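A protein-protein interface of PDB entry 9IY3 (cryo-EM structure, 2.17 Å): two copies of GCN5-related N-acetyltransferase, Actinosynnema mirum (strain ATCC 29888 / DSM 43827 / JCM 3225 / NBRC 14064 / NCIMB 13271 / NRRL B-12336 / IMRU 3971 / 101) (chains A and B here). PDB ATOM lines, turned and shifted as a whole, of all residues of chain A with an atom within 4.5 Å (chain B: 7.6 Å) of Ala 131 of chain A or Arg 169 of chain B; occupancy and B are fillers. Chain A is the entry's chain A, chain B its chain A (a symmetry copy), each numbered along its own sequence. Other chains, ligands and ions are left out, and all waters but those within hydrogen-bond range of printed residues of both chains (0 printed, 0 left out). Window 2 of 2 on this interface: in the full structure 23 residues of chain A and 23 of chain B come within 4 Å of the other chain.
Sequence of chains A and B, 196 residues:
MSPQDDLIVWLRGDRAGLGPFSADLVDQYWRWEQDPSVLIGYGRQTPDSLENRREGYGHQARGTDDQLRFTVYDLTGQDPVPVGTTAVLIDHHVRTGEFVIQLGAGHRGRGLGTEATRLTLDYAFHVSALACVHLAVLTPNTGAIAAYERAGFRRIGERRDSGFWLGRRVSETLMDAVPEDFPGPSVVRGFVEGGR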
ATOM      1  N   VAL A  94     -10.432  23.630   0.445  1.00  0.00           N
ATOM      2  CA  VAL A  94      -9.088  23.248   0.856  1.00  0.00           C
ATOM      3  C   VAL A  94      -8.924  23.194   2.365  1.00  0.00           C
ATOM      4  O   VAL A  94      -7.803  22.996   2.844  1.00  0.00           O
ATOM      5  CB  VAL A  94      -8.028  24.182   0.239  1.00  0.00           C
ATOM      6  CG1 VAL A  94      -7.986  24.007  -1.266  1.00  0.00           C
ATOM      7  CG2 VAL A  94      -8.331  25.623   0.589  1.00  0.00           C
ATOM      8  N   ARG A  95     -10.004  23.364   3.131  1.00  0.00           N
ATOM      9  CA  ARG A  95      -9.965  23.285   4.593  1.00  0.00           C
ATOM     10  C   ARG A  95      -9.031  24.334   5.193  1.00  0.00           C
ATOM     11  O   ARG A  95      -8.271  24.052   6.120  1.00  0.00           O
ATOM     12  CB  ARG A  95      -9.568  21.882   5.067  1.00  0.00           C
ATOM     13  CG  ARG A  95     -10.318  20.731   4.413  1.00  0.00           C
ATOM     14  CD  ARG A  95     -11.812  20.974   4.407  1.00  0.00           C
ATOM     15  NE  ARG A  95     -12.327  21.135   5.760  1.00  0.00           N
ATOM     16  CZ  ARG A  95     -13.531  21.603   6.052  1.00  0.00           C
ATOM     17  NH1 ARG A  95     -14.380  21.960   5.105  1.00  0.00           N
ATOM     18  NH2 ARG A  95     -13.890  21.720   7.326  1.00  0.00           N
ATOM     19  N   ALA A 129     -12.474  21.495  11.643  1.00  0.00           N
ATOM     20  CA  ALA A 129     -11.566  20.576  10.957  1.00  0.00           C
ATOM     21  C   ALA A 129     -10.802  21.277   9.835  1.00  0.00           C
ATOM     22  O   ALA A 129     -10.706  20.786   8.710  1.00  0.00           O
ATOM     23  CB  ALA A 129     -12.320  19.355  10.427  1.00  0.00           C
ATOM     24  N   LEU A 130     -10.251  22.444  10.155  1.00  0.00           N
ATOM     25  CA  LEU A 130      -9.427  23.189   9.215  1.00  0.00           C
ATOM     26  C   LEU A 130      -7.981  22.723   9.304  1.00  0.00           C
ATOM     27  O   LEU A 130      -7.463  22.468  10.395  1.00  0.00           O
ATOM     28  CB  LEU A 130      -9.510  24.692   9.490  1.00  0.00           C
ATOM     29  CG  LEU A 130     -10.901  25.317   9.409  1.00  0.00           C
ATOM     30  CD1 LEU A 130     -10.813  26.825   9.513  1.00  0.00           C
ATOM     31  CD2 LEU A 130     -11.585  24.911   8.121  1.00  0.00           C
ATOM     32  N   ALA A 131      -7.334  22.609   8.146  1.00  0.00           N
ATOM     33  CA  ALA A 131      -5.951  22.162   8.088  1.00  0.00           C
ATOM     34  C   ALA A 131      -4.949  23.298   8.228  1.00  0.00           C
ATOM     35  O   ALA A 131      -3.796  23.043   8.591  1.00  0.00           O
ATOM     36  CB  ALA A 131      -5.690  21.420   6.775  1.00  0.00           C
ATOM     37  N   CYS A 132      -5.355  24.535   7.955  1.00  0.00           N
ATOM     38  CA  CYS A 132      -4.445  25.670   8.028  1.00  0.00           C
ATOM     39  C   CYS A 132      -5.251  26.941   8.235  1.00  0.00           C
ATOM     40  O   CYS A 132      -6.239  27.169   7.534  1.00  0.00           O
ATOM     41  CB  CYS A 132      -3.599  25.780   6.756  1.00  0.00           C
ATOM     42  SG  CYS A 132      -2.392  27.121   6.773  1.00  0.00           S
ATOM     43  N   ALA A 177      -0.989  28.867  10.815  1.00  0.00           N
ATOM     44  CA  ALA A 177      -1.032  27.957  11.949  1.00  0.00           C
ATOM     45  C   ALA A 177      -1.533  26.602  11.482  1.00  0.00           C
ATOM     46  O   ALA A 177      -2.406  26.521  10.614  1.00  0.00           O
ATOM     47  CB  ALA A 177      -1.930  28.497  13.066  1.00  0.00           C
ATOM     48  N   VAL A 178      -0.978  25.541  12.059  1.00  0.00           N
ATOM     49  CA  VAL A 178      -1.360  24.177  11.703  1.00  0.00           C
ATOM     50  C   VAL A 178      -1.740  23.426  12.974  1.00  0.00           C
ATOM     51  O   VAL A 178      -1.266  23.779  14.064  1.00  0.00           O
ATOM     52  CB  VAL A 178      -0.232  23.461  10.943  1.00  0.00           C
ATOM     53  CG1 VAL A 178       0.009  24.134   9.604  1.00  0.00           C
ATOM     54  CG2 VAL A 178       1.041  23.450  11.769  1.00  0.00           C
ATOM     55  N   PRO A 179      -2.602  22.407  12.888  1.00  0.00           N
ATOM     56  CA  PRO A 179      -3.014  21.694  14.109  1.00  0.00           C
ATOM     57  C   PRO A 179      -1.863  21.095  14.897  1.00  0.00           C
ATOM     58  O   PRO A 179      -1.907  21.090  16.134  1.00  0.00           O
ATOM     59  CB  PRO A 179      -3.949  20.609  13.561  1.00  0.00           C
ATOM     60  CG  PRO A 179      -4.539  21.231  12.351  1.00  0.00           C
ATOM     61  CD  PRO A 179      -3.412  22.007  11.725  1.00  0.00           C
ATOM     62  N   PRO B 140       4.174  21.993  -5.853  1.00  0.00           N
ATOM     63  CA  PRO B 140       4.640  21.054  -6.889  1.00  0.00           C
ATOM     64  C   PRO B 140       4.610  21.622  -8.299  1.00  0.00           C
ATOM     65  O   PRO B 140       5.272  21.068  -9.183  1.00  0.00           O
ATOM     66  CB  PRO B 140       3.679  19.869  -6.744  1.00  0.00           C
ATOM     67  CG  PRO B 140       3.211  19.945  -5.341  1.00  0.00           C
ATOM     68  CD  PRO B 140       3.059  21.410  -5.083  1.00  0.00           C
ATOM     69  N   ARG B 160       1.877  26.465   4.718  1.00  0.00           N
ATOM     70  CA  ARG B 160       1.829  25.026   4.941  1.00  0.00           C
ATOM     71  C   ARG B 160       0.403  24.490   4.887  1.00  0.00           C
ATOM     72  O   ARG B 160      -0.518  25.066   5.471  1.00  0.00           O
ATOM     73  CB  ARG B 160       2.451  24.688   6.293  1.00  0.00           C
ATOM     74  CG  ARG B 160       3.935  24.970   6.384  1.00  0.00           C
ATOM     75  CD  ARG B 160       4.418  24.790   7.808  1.00  0.00           C
ATOM     76  NE  ARG B 160       3.786  25.748   8.706  1.00  0.00           N
ATOM     77  CZ  ARG B 160       3.847  25.690  10.028  1.00  0.00           C
ATOM     78  NH1 ARG B 160       4.500  24.721  10.648  1.00  0.00           N
ATOM     79  NH2 ARG B 160       3.235  26.626  10.748  1.00  0.00           N
ATOM     80  N   ASP B 161       0.237  23.368   4.187  1.00  0.00           N
ATOM     81  CA  ASP B 161      -0.989  22.570   4.189  1.00  0.00           C
ATOM     82  C   ASP B 161      -2.221  23.419   3.871  1.00  0.00           C
ATOM     83  O   ASP B 161      -3.165  23.516   4.654  1.00  0.00           O
ATOM     84  CB  ASP B 161      -1.156  21.847   5.528  1.00  0.00           C
ATOM     85  CG  ASP B 161       0.007  20.928   5.843  1.00  0.00           C
ATOM     86  OD1 ASP B 161       0.808  20.646   4.929  1.00  0.00           O
ATOM     87  OD2 ASP B 161       0.121  20.487   7.005  1.00  0.00           O
ATOM     88  N   SER B 162      -2.198  24.037   2.690  1.00  0.00           N
ATOM     89  CA  SER B 162      -3.307  24.880   2.259  1.00  0.00           C
ATOM     90  C   SER B 162      -3.739  24.580   0.827  1.00  0.00           C
ATOM     91  O   SER B 162      -4.356  25.432   0.182  1.00  0.00           O
ATOM     92  CB  SER B 162      -2.949  26.360   2.401  1.00  0.00           C
ATOM     93  OG  SER B 162      -1.906  26.714   1.516  1.00  0.00           O
ATOM     94  N   GLY B 163      -3.440  23.389   0.321  1.00  0.00           N
ATOM     95  CA  GLY B 163      -3.849  23.034  -1.025  1.00  0.00           C
ATOM     96  C   GLY B 163      -3.683  21.551  -1.260  1.00  0.00           C
ATOM     97  O   GLY B 163      -3.046  20.841  -0.478  1.00  0.00           O
ATOM     98  N   PHE B 164      -4.274  21.093  -2.360  1.00  0.00           N
ATOM     99  CA  PHE B 164      -4.230  19.694  -2.758  1.00  0.00           C
ATOM    100  C   PHE B 164      -3.542  19.570  -4.107  1.00  0.00           C
ATOM    101  O   PHE B 164      -3.826  20.345  -5.026  1.00  0.00           O
ATOM    102  CB  PHE B 164      -5.636  19.090  -2.836  1.00  0.00           C
ATOM    103  CG  PHE B 164      -6.301  18.919  -1.502  1.00  0.00           C
ATOM    104  CD1 PHE B 164      -6.048  17.801  -0.729  1.00  0.00           C
ATOM    105  CD2 PHE B 164      -7.195  19.863  -1.032  1.00  0.00           C
ATOM    106  CE1 PHE B 164      -6.660  17.635   0.495  1.00  0.00           C
ATOM    107  CE2 PHE B 164      -7.812  19.701   0.190  1.00  0.00           C
ATOM    108  CZ  PHE B 164      -7.544  18.586   0.953  1.00  0.00           C
ATOM    109  N   TRP B 165      -2.637  18.601  -4.222  1.00  0.00           N
ATOM    110  CA  TRP B 165      -1.992  18.268  -5.489  1.00  0.00           C
ATOM    111  C   TRP B 165      -2.158  16.772  -5.714  1.00  0.00           C
ATOM    112  O   TRP B 165      -1.515  15.966  -5.034  1.00  0.00           O
ATOM    113  CB  TRP B 165      -0.518  18.669  -5.485  1.00  0.00           C
ATOM    114  CG  TRP B 165       0.163  18.473  -6.803  1.00  0.00           C
ATOM    115  CD1 TRP B 165       0.830  17.363  -7.226  1.00  0.00           C
ATOM    116  CD2 TRP B 165       0.226  19.413  -7.882  1.00  0.00           C
ATOM    117  NE1 TRP B 165       1.315  17.556  -8.495  1.00  0.00           N
ATOM    118  CE2 TRP B 165       0.956  18.807  -8.921  1.00  0.00           C
ATOM    119  CE3 TRP B 165      -0.259  20.710  -8.067  1.00  0.00           C
ATOM    120  CZ2 TRP B 165       1.211  19.453 -10.127  1.00  0.00           C
ATOM    121  CZ3 TRP B 165      -0.005  21.349  -9.264  1.00  0.00           C
ATOM    122  CH2 TRP B 165       0.722  20.720 -10.278  1.00  0.00           C
ATOM    123  N   LEU B 166      -3.016  16.408  -6.669  1.00  0.00           N
ATOM    124  CA  LEU B 166      -3.354  15.010  -6.945  1.00  0.00           C
ATOM    125  C   LEU B 166      -3.853  14.302  -5.687  1.00  0.00           C
ATOM    126  O   LEU B 166      -3.505  13.151  -5.421  1.00  0.00           O
ATOM    127  CB  LEU B 166      -2.171  14.260  -7.559  1.00  0.00           C
ATOM    128  CG  LEU B 166      -1.593  14.840  -8.850  1.00  0.00           C
ATOM    129  CD1 LEU B 166      -0.384  14.041  -9.298  1.00  0.00           C
ATOM    130  CD2 LEU B 166      -2.649  14.874  -9.939  1.00  0.00           C
ATOM    131  N   GLY B 167      -4.671  15.002  -4.903  1.00  0.00           N
ATOM    132  CA  GLY B 167      -5.238  14.447  -3.694  1.00  0.00           C
ATOM    133  C   GLY B 167      -4.353  14.524  -2.473  1.00  0.00           C
ATOM    134  O   GLY B 167      -4.822  14.223  -1.369  1.00  0.00           O
ATOM    135  N   ARG B 168      -3.093  14.914  -2.628  1.00  0.00           N
ATOM    136  CA  ARG B 168      -2.159  15.000  -1.518  1.00  0.00           C
ATOM    137  C   ARG B 168      -2.126  16.419  -0.968  1.00  0.00           C
ATOM    138  O   ARG B 168      -2.107  17.393  -1.726  1.00  0.00           O
ATOM    139  CB  ARG B 168      -0.763  14.570  -1.971  1.00  0.00           C
ATOM    140  CG  ARG B 168       0.306  14.625  -0.897  1.00  0.00           C
ATOM    141  CD  ARG B 168       1.560  13.898  -1.358  1.00  0.00           C
ATOM    142  NE  ARG B 168       2.114  14.483  -2.572  1.00  0.00           N
ATOM    143  CZ  ARG B 168       3.028  15.443  -2.594  1.00  0.00           C
ATOM    144  NH1 ARG B 168       3.527  15.949  -1.478  1.00  0.00           N
ATOM    145  NH2 ARG B 168       3.455  15.906  -3.766  1.00  0.00           N
ATOM    146  N   ARG B 169      -2.129  16.531   0.358  1.00  0.00           N
ATOM    147  CA  ARG B 169      -2.070  17.835   1.006  1.00  0.00           C
ATOM    148  C   ARG B 169      -0.663  18.407   0.891  1.00  0.00           C
ATOM    149  O   ARG B 169       0.294  17.829   1.414  1.00  0.00           O
ATOM    150  CB  ARG B 169      -2.488  17.713   2.468  1.00  0.00           C
ATOM    151  CG  ARG B 169      -2.382  19.001   3.259  1.00  0.00           C
ATOM    152  CD  ARG B 169      -3.518  19.953   2.943  1.00  0.00           C
ATOM    153  NE  ARG B 169      -4.776  19.539   3.549  1.00  0.00           N
ATOM    154  CZ  ARG B 169      -5.896  20.245   3.498  1.00  0.00           C
ATOM    155  NH1 ARG B 169      -5.946  21.418   2.889  1.00  0.00           N
ATOM    156  NH2 ARG B 169      -6.993  19.764   4.074  1.00  0.00           N
ATOM    157  N   VAL B 170      -0.540  19.546   0.208  1.00  0.00           N
ATOM    158  CA  VAL B 170       0.742  20.189  -0.038  1.00  0.00           C
ATOM    159  C   VAL B 170       0.620  21.669   0.300  1.00  0.00           C
ATOM    160  O   VAL B 170      -0.476  22.217   0.415  1.00  0.00           O
ATOM    161  CB  VAL B 170       1.221  20.011  -1.494  1.00  0.00           C
ATOM    162  CG1 VAL B 170       1.425  18.543  -1.817  1.00  0.00           C
ATOM    163  CG2 VAL B 170       0.228  20.641  -2.454  1.00  0.00           C
ATOM    164  N   SER B 171       1.772  22.312   0.458  1.00  0.00           N
ATOM    165  CA  SER B 171       1.823  23.746   0.682  1.00  0.00           C
ATOM    166  C   SER B 171       1.782  24.491  -0.651  1.00  0.00           C
ATOM    167  O   SER B 171       1.938  23.906  -1.726  1.00  0.00           O
ATOM    168  CB  SER B 171       3.079  24.121   1.462  1.00  0.00           C
ATOM    169  OG  SER B 171       4.243  23.892   0.688  1.00  0.00           O
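N of Ser 162 of chain B sits at hydrogen-bond distance from O of Val 170 of chain B (3.4 Å). The backbone NH (N) of Ala 131 of chain A sits at hydrogen-bond distance from the backbone carbonyl oxygen (O) of Arg 95 of chain A (2.7 Å). N of Cys 132 of chain A is in hydrogen-bond range of O of Arg 95 of chain A (3.5 Å). NE of Arg 95 of chain A is in hydrogen-bond range of O of Ala 129 of chain A.
The guanidinium group of Arg 169 of chain B lies within hydrogen-bond range of the backbone carbonyl oxygen of Val 94 of chain A, at 2.4 Å. The side-chain sulfur (SG) of Cys 132 of chain A sits at hydrogen-bond distance from the backbone carbonyl oxygen (O) of Arg 160 of chain B.
No position is printed for both chains. Of the 9 pairs that touch across the chains among the printed residues, none has its exchanged pair printed and touching as well.
Among the printed residues, pairs that only touch across the chains: Val 94 of chain A with Ser 162 of chain B (3.9 Å), Val 94 of chain A with Phe 164 of chain B (3.8 Å), Arg 95 of chain A with Arg 169 of chain B (3.5 Å), Ala 131 of chain A with Asp 161 of chain B (3.9 Å), Ala 131 of chain A with Arg 169 of chain B (3.4 Å), Cys 132 of chain A with Asp 161 of chain B (3.1 Å) and Val 178 of chain A with Arg 160 of chain B (3.9 Å).
Of the 13 printed residues of chain B, 5 touch a printed residue of chain A. Printed residues of chain B that touch a printed residue of chain A: Arg 160, Asp 161, Ser 162, Phe 164 and Arg 169.
Ala 131 of chain A touches just these residues of chain B: Asp 161 (3.9 Å) and Arg 169 (3.4 Å). Of chain A, only Val 94, Arg 95 and Ala 131 come within 4 Å of Arg 169 of chain B. Of the printed residues of chain B, Cys 132 of chain A touches Arg 160 (3.1 Å) and Asp 161 (3.1 Å). Printed residues of chain B within 4 Å of Val 94 of chain A: Ser 162 (3.9 Å), Phe 164 (3.8 Å) and Arg 169 (2.4 Å). The nearest residue of chain B that does not touch Ala 131 of chain A is Arg 160 of chain B (5.0 Å). The nearest printed residue of chain A that does not touch Arg 169 of chain B is Cys 132 of chain A (6.0 Å). The nearest printed residue of chain A that does not touch Arg 160 of chain B is Ala 177 of chain A (4.6 Å).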
